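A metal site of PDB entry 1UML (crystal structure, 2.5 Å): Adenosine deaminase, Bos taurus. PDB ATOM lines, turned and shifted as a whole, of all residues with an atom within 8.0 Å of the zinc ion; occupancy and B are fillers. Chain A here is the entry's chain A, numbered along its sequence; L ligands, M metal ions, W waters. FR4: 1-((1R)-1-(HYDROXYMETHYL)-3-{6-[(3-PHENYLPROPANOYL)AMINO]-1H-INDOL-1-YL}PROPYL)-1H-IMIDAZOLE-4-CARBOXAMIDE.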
ATOM      1  N   HIS A  14       8.909 -33.181 -14.304  1.00  0.00           N
ATOM      2  CA  HIS A  14       9.178 -32.394 -13.113  1.00  0.00           C
ATOM      3  C   HIS A  14       7.932 -31.686 -12.581  1.00  0.00           C
ATOM      4  O   HIS A  14       7.612 -30.539 -12.871  1.00  0.00           O
ATOM      5  CB  HIS A  14      10.404 -31.483 -13.360  1.00  0.00           C
ATOM      6  CG  HIS A  14      10.903 -30.802 -12.092  1.00  0.00           C
ATOM      7  ND1 HIS A  14      12.174 -30.862 -11.664  1.00  0.00           N
ATOM      8  CD2 HIS A  14      10.182 -30.056 -11.164  1.00  0.00           C
ATOM      9  CE1 HIS A  14      12.280 -30.194 -10.487  1.00  0.00           C
ATOM     10  NE2 HIS A  14      11.042 -29.699 -10.185  1.00  0.00           N
ATOM     11  N   VAL A  15       7.257 -32.466 -11.709  1.00  0.00           N
ATOM     12  CA  VAL A  15       6.075 -31.918 -11.043  1.00  0.00           C
ATOM     13  C   VAL A  15       5.845 -32.573  -9.692  1.00  0.00           C
ATOM     14  O   VAL A  15       6.006 -33.776  -9.509  1.00  0.00           O
ATOM     15  CB  VAL A  15       4.832 -31.960 -11.967  1.00  0.00           C
ATOM     16  CG1 VAL A  15       4.629 -33.336 -12.586  1.00  0.00           C
ATOM     17  CG2 VAL A  15       3.573 -31.389 -11.301  1.00  0.00           C
ATOM     18  N   HIS A  16       5.508 -31.665  -8.747  1.00  0.00           N
ATOM     19  CA  HIS A  16       5.298 -32.095  -7.367  1.00  0.00           C
ATOM     20  C   HIS A  16       3.848 -32.385  -7.088  1.00  0.00           C
ATOM     21  O   HIS A  16       2.970 -31.561  -7.311  1.00  0.00           O
ATOM     22  CB  HIS A  16       5.768 -31.031  -6.393  1.00  0.00           C
ATOM     23  CG  HIS A  16       7.266 -30.819  -6.400  1.00  0.00           C
ATOM     24  ND1 HIS A  16       8.081 -31.341  -5.496  1.00  0.00           N
ATOM     25  CD2 HIS A  16       8.014 -29.980  -7.226  1.00  0.00           C
ATOM     26  CE1 HIS A  16       9.332 -30.846  -5.726  1.00  0.00           C
ATOM     27  NE2 HIS A  16       9.288 -30.010  -6.784  1.00  0.00           N
ATOM     28  N   PHE A  60       6.454 -18.455   0.791  1.00  0.00           N
ATOM     29  CA  PHE A  60       6.243 -19.701   0.039  1.00  0.00           C
ATOM     30  C   PHE A  60       5.810 -20.911   0.864  1.00  0.00           C
ATOM     31  O   PHE A  60       4.838 -21.568   0.545  1.00  0.00           O
ATOM     32  CB  PHE A  60       7.523 -20.001  -0.790  1.00  0.00           C
ATOM     33  CG  PHE A  60       7.421 -21.238  -1.668  1.00  0.00           C
ATOM     34  CD1 PHE A  60       6.527 -21.246  -2.768  1.00  0.00           C
ATOM     35  CD2 PHE A  60       8.214 -22.360  -1.364  1.00  0.00           C
ATOM     36  CE1 PHE A  60       6.446 -22.390  -3.585  1.00  0.00           C
ATOM     37  CE2 PHE A  60       8.136 -23.511  -2.187  1.00  0.00           C
ATOM     38  CZ  PHE A  60       7.270 -23.505  -3.308  1.00  0.00           C
ATOM     39  N   ARG A 100       6.714 -36.267  -8.497  1.00  0.00           N
ATOM     40  CA  ARG A 100       7.548 -36.404  -7.311  1.00  0.00           C
ATOM     41  C   ARG A 100       6.910 -35.898  -6.041  1.00  0.00           C
ATOM     42  O   ARG A 100       6.103 -34.960  -6.020  1.00  0.00           O
ATOM     43  CB  ARG A 100       8.928 -35.773  -7.549  1.00  0.00           C
ATOM     44  CG  ARG A 100       8.932 -34.242  -7.544  1.00  0.00           C
ATOM     45  CD  ARG A 100       9.708 -33.647  -8.705  1.00  0.00           C
ATOM     46  NE  ARG A 100      11.115 -33.991  -8.660  1.00  0.00           N
ATOM     47  CZ  ARG A 100      11.887 -34.009  -9.756  1.00  0.00           C
ATOM     48  NH1 ARG A 100      13.154 -33.685  -9.629  1.00  0.00           N
ATOM     49  NH2 ARG A 100      11.414 -34.333 -10.957  1.00  0.00           N
ATOM     50  N   CYS A 152      11.178 -37.883  -3.171  1.00  0.00           N
ATOM     51  CA  CYS A 152      12.077 -36.825  -2.703  1.00  0.00           C
ATOM     52  C   CYS A 152      12.675 -37.082  -1.331  1.00  0.00           C
ATOM     53  O   CYS A 152      11.952 -37.324  -0.387  1.00  0.00           O
ATOM     54  CB  CYS A 152      11.347 -35.492  -2.621  1.00  0.00           C
ATOM     55  SG  CYS A 152      10.580 -35.022  -4.176  1.00  0.00           S
ATOM     56  N   ASP A 180      15.034 -38.308  -5.594  1.00  0.00           N
ATOM     57  CA  ASP A 180      15.275 -36.882  -5.742  1.00  0.00           C
ATOM     58  C   ASP A 180      15.764 -36.283  -4.426  1.00  0.00           C
ATOM     59  O   ASP A 180      15.753 -36.925  -3.388  1.00  0.00           O
ATOM     60  CB  ASP A 180      14.011 -36.222  -6.300  1.00  0.00           C
ATOM     61  CG  ASP A 180      14.115 -34.714  -6.535  1.00  0.00           C
ATOM     62  OD1 ASP A 180      13.132 -34.026  -6.252  1.00  0.00           O
ATOM     63  OD2 ASP A 180      15.147 -34.226  -6.983  1.00  0.00           O
ATOM     64  N   LEU A 181      16.232 -35.030  -4.531  1.00  0.00           N
ATOM     65  CA  LEU A 181      16.646 -34.280  -3.375  1.00  0.00           C
ATOM     66  C   LEU A 181      16.074 -32.886  -3.511  1.00  0.00           C
ATOM     67  O   LEU A 181      16.301 -32.188  -4.481  1.00  0.00           O
ATOM     68  CB  LEU A 181      18.164 -34.337  -3.302  1.00  0.00           C
ATOM     69  CG  LEU A 181      18.952 -33.965  -2.041  1.00  0.00           C
ATOM     70  CD1 LEU A 181      19.811 -32.787  -2.382  1.00  0.00           C
ATOM     71  CD2 LEU A 181      18.173 -33.764  -0.741  1.00  0.00           C
ATOM     72  N   ALA A 182      15.267 -32.551  -2.495  1.00  0.00           N
ATOM     73  CA  ALA A 182      14.481 -31.339  -2.607  1.00  0.00           C
ATOM     74  C   ALA A 182      14.559 -30.515  -1.338  1.00  0.00           C
ATOM     75  O   ALA A 182      15.063 -30.967  -0.304  1.00  0.00           O
ATOM     76  CB  ALA A 182      13.015 -31.710  -2.940  1.00  0.00           C
ATOM     77  N   GLY A 183      14.061 -29.281  -1.488  1.00  0.00           N
ATOM     78  CA  GLY A 183      13.856 -28.342  -0.384  1.00  0.00           C
ATOM     79  C   GLY A 183      15.009 -27.553   0.226  1.00  0.00           C
ATOM     80  O   GLY A 183      15.439 -27.852   1.335  1.00  0.00           O
ATOM     81  N   HIS A 213      17.634 -31.507  -7.294  1.00  0.00           N
ATOM     82  CA  HIS A 213      17.239 -30.125  -7.530  1.00  0.00           C
ATOM     83  C   HIS A 213      18.245 -29.002  -7.730  1.00  0.00           C
ATOM     84  O   HIS A 213      17.885 -28.017  -8.341  1.00  0.00           O
ATOM     85  CB  HIS A 213      16.295 -29.652  -6.469  1.00  0.00           C
ATOM     86  CG  HIS A 213      14.884 -30.035  -6.743  1.00  0.00           C
ATOM     87  ND1 HIS A 213      14.310 -31.144  -6.264  1.00  0.00           N
ATOM     88  CD2 HIS A 213      13.925 -29.262  -7.379  1.00  0.00           C
ATOM     89  CE1 HIS A 213      12.995 -31.090  -6.572  1.00  0.00           C
ATOM     90  NE2 HIS A 213      12.761 -29.932  -7.254  1.00  0.00           N
ATOM     91  N   GLU A 216      18.586 -23.984  -8.860  1.00  0.00           N
ATOM     92  CA  GLU A 216      17.542 -22.978  -9.090  1.00  0.00           C
ATOM     93  C   GLU A 216      17.846 -21.689  -8.397  1.00  0.00           C
ATOM     94  O   GLU A 216      17.832 -20.614  -8.985  1.00  0.00           O
ATOM     95  CB  GLU A 216      16.084 -23.425  -8.803  1.00  0.00           C
ATOM     96  CG  GLU A 216      15.757 -24.021  -7.438  1.00  0.00           C
ATOM     97  CD  GLU A 216      14.254 -24.240  -7.206  1.00  0.00           C
ATOM     98  OE1 GLU A 216      13.904 -25.253  -6.606  1.00  0.00           O
ATOM     99  OE2 GLU A 216      13.444 -23.392  -7.595  1.00  0.00           O
ATOM    100  N   GLY A 236      17.170 -31.152 -11.750  1.00  0.00           N
ATOM    101  CA  GLY A 236      16.029 -30.243 -11.654  1.00  0.00           C
ATOM    102  C   GLY A 236      16.485 -28.801 -11.634  1.00  0.00           C
ATOM    103  O   GLY A 236      17.225 -28.418 -10.746  1.00  0.00           O
ATOM    104  N   HIS A 237      16.033 -28.054 -12.661  1.00  0.00           N
ATOM    105  CA  HIS A 237      16.423 -26.654 -12.889  1.00  0.00           C
ATOM    106  C   HIS A 237      17.812 -26.437 -13.510  1.00  0.00           C
ATOM    107  O   HIS A 237      17.963 -26.278 -14.712  1.00  0.00           O
ATOM    108  CB  HIS A 237      16.238 -25.779 -11.645  1.00  0.00           C
ATOM    109  CG  HIS A 237      14.820 -25.821 -11.107  1.00  0.00           C
ATOM    110  ND1 HIS A 237      13.795 -25.104 -11.604  1.00  0.00           N
ATOM    111  CD2 HIS A 237      14.351 -26.560 -10.019  1.00  0.00           C
ATOM    112  CE1 HIS A 237      12.683 -25.375 -10.847  1.00  0.00           C
ATOM    113  NE2 HIS A 237      13.034 -26.271  -9.883  1.00  0.00           N
ATOM    114  N   GLU A 259      15.857 -30.377 -16.224  1.00  0.00           N
ATOM    115  CA  GLU A 259      14.426 -30.195 -16.010  1.00  0.00           C
ATOM    116  C   GLU A 259      14.052 -28.719 -15.799  1.00  0.00           C
ATOM    117  O   GLU A 259      14.112 -28.183 -14.697  1.00  0.00           O
ATOM    118  CB  GLU A 259      14.014 -31.055 -14.809  1.00  0.00           C
ATOM    119  CG  GLU A 259      14.462 -32.512 -14.873  1.00  0.00           C
ATOM    120  CD  GLU A 259      14.396 -33.227 -13.517  1.00  0.00           C
ATOM    121  OE1 GLU A 259      14.927 -34.320 -13.409  1.00  0.00           O
ATOM    122  OE2 GLU A 259      13.849 -32.702 -12.562  1.00  0.00           O
ATOM    123  N   CYS A 261      11.844 -25.378 -15.439  1.00  0.00           N
ATOM    124  CA  CYS A 261      10.514 -24.924 -15.047  1.00  0.00           C
ATOM    125  C   CYS A 261      10.394 -23.403 -15.139  1.00  0.00           C
ATOM    126  O   CYS A 261      10.637 -22.683 -14.180  1.00  0.00           O
ATOM    127  CB  CYS A 261      10.181 -25.395 -13.641  1.00  0.00           C
ATOM    128  SG  CYS A 261      10.553 -27.139 -13.297  1.00  0.00           S
ATOM    129  N   SER A 264       7.687 -21.269 -12.913  1.00  0.00           N
ATOM    130  CA  SER A 264       8.210 -21.354 -11.558  1.00  0.00           C
ATOM    131  C   SER A 264       9.326 -20.376 -11.254  1.00  0.00           C
ATOM    132  O   SER A 264       9.326 -19.743 -10.219  1.00  0.00           O
ATOM    133  CB  SER A 264       8.639 -22.795 -11.283  1.00  0.00           C
ATOM    134  OG  SER A 264       9.121 -22.969  -9.937  1.00  0.00           O
ATOM    135  N   THR A 293       6.064 -27.971 -15.097  1.00  0.00           N
ATOM    136  CA  THR A 293       5.079 -27.080 -14.481  1.00  0.00           C
ATOM    137  C   THR A 293       5.395 -26.770 -13.019  1.00  0.00           C
ATOM    138  O   THR A 293       5.045 -25.725 -12.490  1.00  0.00           O
ATOM    139  CB  THR A 293       3.699 -27.762 -14.700  1.00  0.00           C
ATOM    140  OG1 THR A 293       2.673 -26.857 -15.097  1.00  0.00           O
ATOM    141  CG2 THR A 293       3.248 -28.684 -13.607  1.00  0.00           C
ATOM    142  N   ASP A 294       6.118 -27.746 -12.412  1.00  0.00           N
ATOM    143  CA  ASP A 294       6.571 -27.683 -11.025  1.00  0.00           C
ATOM    144  C   ASP A 294       5.474 -27.807  -9.994  1.00  0.00           C
ATOM    145  O   ASP A 294       5.266 -28.862  -9.421  1.00  0.00           O
ATOM    146  CB  ASP A 294       7.485 -26.464 -10.820  1.00  0.00           C
ATOM    147  CG  ASP A 294       8.591 -26.685  -9.800  1.00  0.00           C
ATOM    148  OD1 ASP A 294       9.395 -25.788  -9.613  1.00  0.00           O
ATOM    149  OD2 ASP A 294       8.653 -27.749  -9.203  1.00  0.00           O
ATOM    150  N   ASP A 295       4.787 -26.678  -9.768  1.00  0.00           N
ATOM    151  CA  ASP A 295       3.684 -26.636  -8.796  1.00  0.00           C
ATOM    152  C   ASP A 295       2.471 -25.889  -9.371  1.00  0.00           C
ATOM    153  O   ASP A 295       2.300 -24.697  -9.142  1.00  0.00           O
ATOM    154  CB  ASP A 295       4.055 -25.938  -7.477  1.00  0.00           C
ATOM    155  CG  ASP A 295       5.347 -26.448  -6.859  1.00  0.00           C
ATOM    156  OD1 ASP A 295       5.275 -27.271  -5.958  1.00  0.00           O
ATOM    157  OD2 ASP A 295       6.411 -26.004  -7.268  1.00  0.00           O
ATOM    158  N   PHE A 299       1.471 -22.169  -8.411  1.00  0.00           N
ATOM    159  CA  PHE A 299       1.720 -21.147  -9.442  1.00  0.00           C
ATOM    160  C   PHE A 299       0.553 -20.844 -10.377  1.00  0.00           C
ATOM    161  O   PHE A 299       0.733 -20.235 -11.427  1.00  0.00           O
ATOM    162  CB  PHE A 299       2.988 -21.476 -10.258  1.00  0.00           C
ATOM    163  CG  PHE A 299       4.185 -21.813  -9.399  1.00  0.00           C
ATOM    164  CD1 PHE A 299       4.505 -21.021  -8.258  1.00  0.00           C
ATOM    165  CD2 PHE A 299       4.967 -22.933  -9.742  1.00  0.00           C
ATOM    166  CE1 PHE A 299       5.580 -21.405  -7.433  1.00  0.00           C
ATOM    167  CE2 PHE A 299       6.056 -23.303  -8.928  1.00  0.00           C
ATOM    168  CZ  PHE A 299       6.337 -22.546  -7.761  1.00  0.00           C
HETATM  169  C1  FR4 L   1       8.973 -28.567  -2.856  1.00  0.00           C
HETATM  170  N2  FR4 L   1       7.798 -29.374  -2.514  1.00  0.00           N
HETATM  171  C3  FR4 L   1       6.773 -29.078  -3.336  1.00  0.00           C
HETATM  172  N4  FR4 L   1       7.170 -28.137  -4.193  1.00  0.00           N
HETATM  173  C5  FR4 L   1       8.548 -27.802  -3.875  1.00  0.00           C
HETATM  174  C8  FR4 L   1       9.346 -26.769  -4.568  1.00  0.00           C
HETATM  175  O9  FR4 L   1      10.400 -26.430  -4.061  1.00  0.00           O
HETATM  176  N10 FR4 L   1       8.889 -26.238  -5.696  1.00  0.00           N
HETATM  177  C13 FR4 L   1       7.730 -30.373  -1.456  1.00  0.00           C
HETATM  178  C14 FR4 L   1       8.210 -31.749  -1.959  1.00  0.00           C
HETATM  179  O15 FR4 L   1       7.481 -32.209  -3.064  1.00  0.00           O
HETATM  180  C18 FR4 L   1       8.461 -29.932  -0.176  1.00  0.00           C
HETATM  181  C19 FR4 L   1       8.095 -28.527   0.329  1.00  0.00           C
HETATM  182  N22 FR4 L   1       9.124 -28.044   1.248  1.00  0.00           N
HETATM  183  C27 FR4 L   1       9.299 -28.369   2.567  1.00  0.00           C
HETATM  184  C28 FR4 L   1      10.428 -27.719   3.074  1.00  0.00           C
HETATM  185  C29 FR4 L   1      10.968 -26.954   1.987  1.00  0.00           C
HETATM  186  C30 FR4 L   1      10.129 -27.182   0.856  1.00  0.00           C
HETATM  187  C31 FR4 L   1      12.055 -26.130   1.884  1.00  0.00           C
HETATM  188  C32 FR4 L   1      12.327 -25.510   0.663  1.00  0.00           C
HETATM  189  C33 FR4 L   1      11.507 -25.736  -0.462  1.00  0.00           C
HETATM  190  C34 FR4 L   1      10.405 -26.580  -0.339  1.00  0.00           C
HETATM  191  N1  FR4 L   1      11.752 -25.181  -1.679  1.00  0.00           N
HETATM  192  C2  FR4 L   1      12.704 -24.263  -1.968  1.00  0.00           C
HETATM  193  O1  FR4 L   1      13.483 -23.743  -1.166  1.00  0.00           O
HETATM  194  C4  FR4 L   1      12.707 -23.935  -3.455  1.00  0.00           C
HETATM  195  C6  FR4 L   1      13.414 -22.606  -3.742  1.00  0.00           C
HETATM  196  C7  FR4 L   1      11.198 -21.373  -3.688  1.00  0.00           C
HETATM  197  C11 FR4 L   1      12.556 -21.404  -3.389  1.00  0.00           C
HETATM  198  C9  FR4 L   1      13.158 -20.297  -2.792  1.00  0.00           C
HETATM  199  C12 FR4 L   1      12.402 -19.161  -2.525  1.00  0.00           C
HETATM  200  C10 FR4 L   1      11.056 -19.125  -2.858  1.00  0.00           C
HETATM  201  C15 FR4 L   1      10.449 -20.232  -3.441  1.00  0.00           C
HETATM  202 ZN    ZN M   1      10.684 -28.914  -8.054  1.00  0.00          ZN
HETATM  203  O   HOH W   1      11.551 -26.898  -7.145  1.00  0.00           O
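ND1 of His 16 sits at hydrogen-bond distance from O15 of the ligand (2.7 Å).
OD1 of Asp 295 is in hydrogen-bond range of N4 of the ligand (2.7 Å).
A ring nitrogen (ND1) of His 14 is in hydrogen-bond range of the side-chain carboxylate (OE2) of Glu 259 (2.6 Å).
OD1 of Asp 180 lies close to ND1 of His 213 (3.1 Å).
The backbone carbonyl oxygen of His 213 lies close to the backbone carbonyl oxygen of Gly 236 (2.5 Å).
A ring nitrogen (ND1) of His 213 is in hydrogen-bond range of the backbone carbonyl oxygen of Leu 181, 2.9 Å away.
The side-chain carboxylate (OD1) of Asp 294 lies within hydrogen-bond range of the side-chain hydroxyl (OG) of Ser 264.
N of His 237 lies within hydrogen-bond range of O of Glu 259 (2.8 Å).
His 237 touches the zinc ion.
Within 4 Å of the zinc ion: His 14, His 16, His 213, His 237 and Asp 294.
The nearest printed residue that does not touch the zinc ion is Arg 100 (4.9 Å).
The zinc ion is bound by NE2 of His 16 (2.2 Å), NE2 of His 14 (2.3 Å), water W1 (2.4 Å), NE2 of His 213 (2.4 Å) and OD2 of Asp 294 (2.6 Å).
Water W1 lies within hydrogen-bond range of the side-chain carboxylate (OE1) of Glu 216 (2.9 Å), a nitrogen (N10) of the ligand (3.1 Å), a ring nitrogen (NE2) of His 237 (3.2 Å) and the side-chain carboxylate (OD1) of Asp 294 (3.5 Å).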
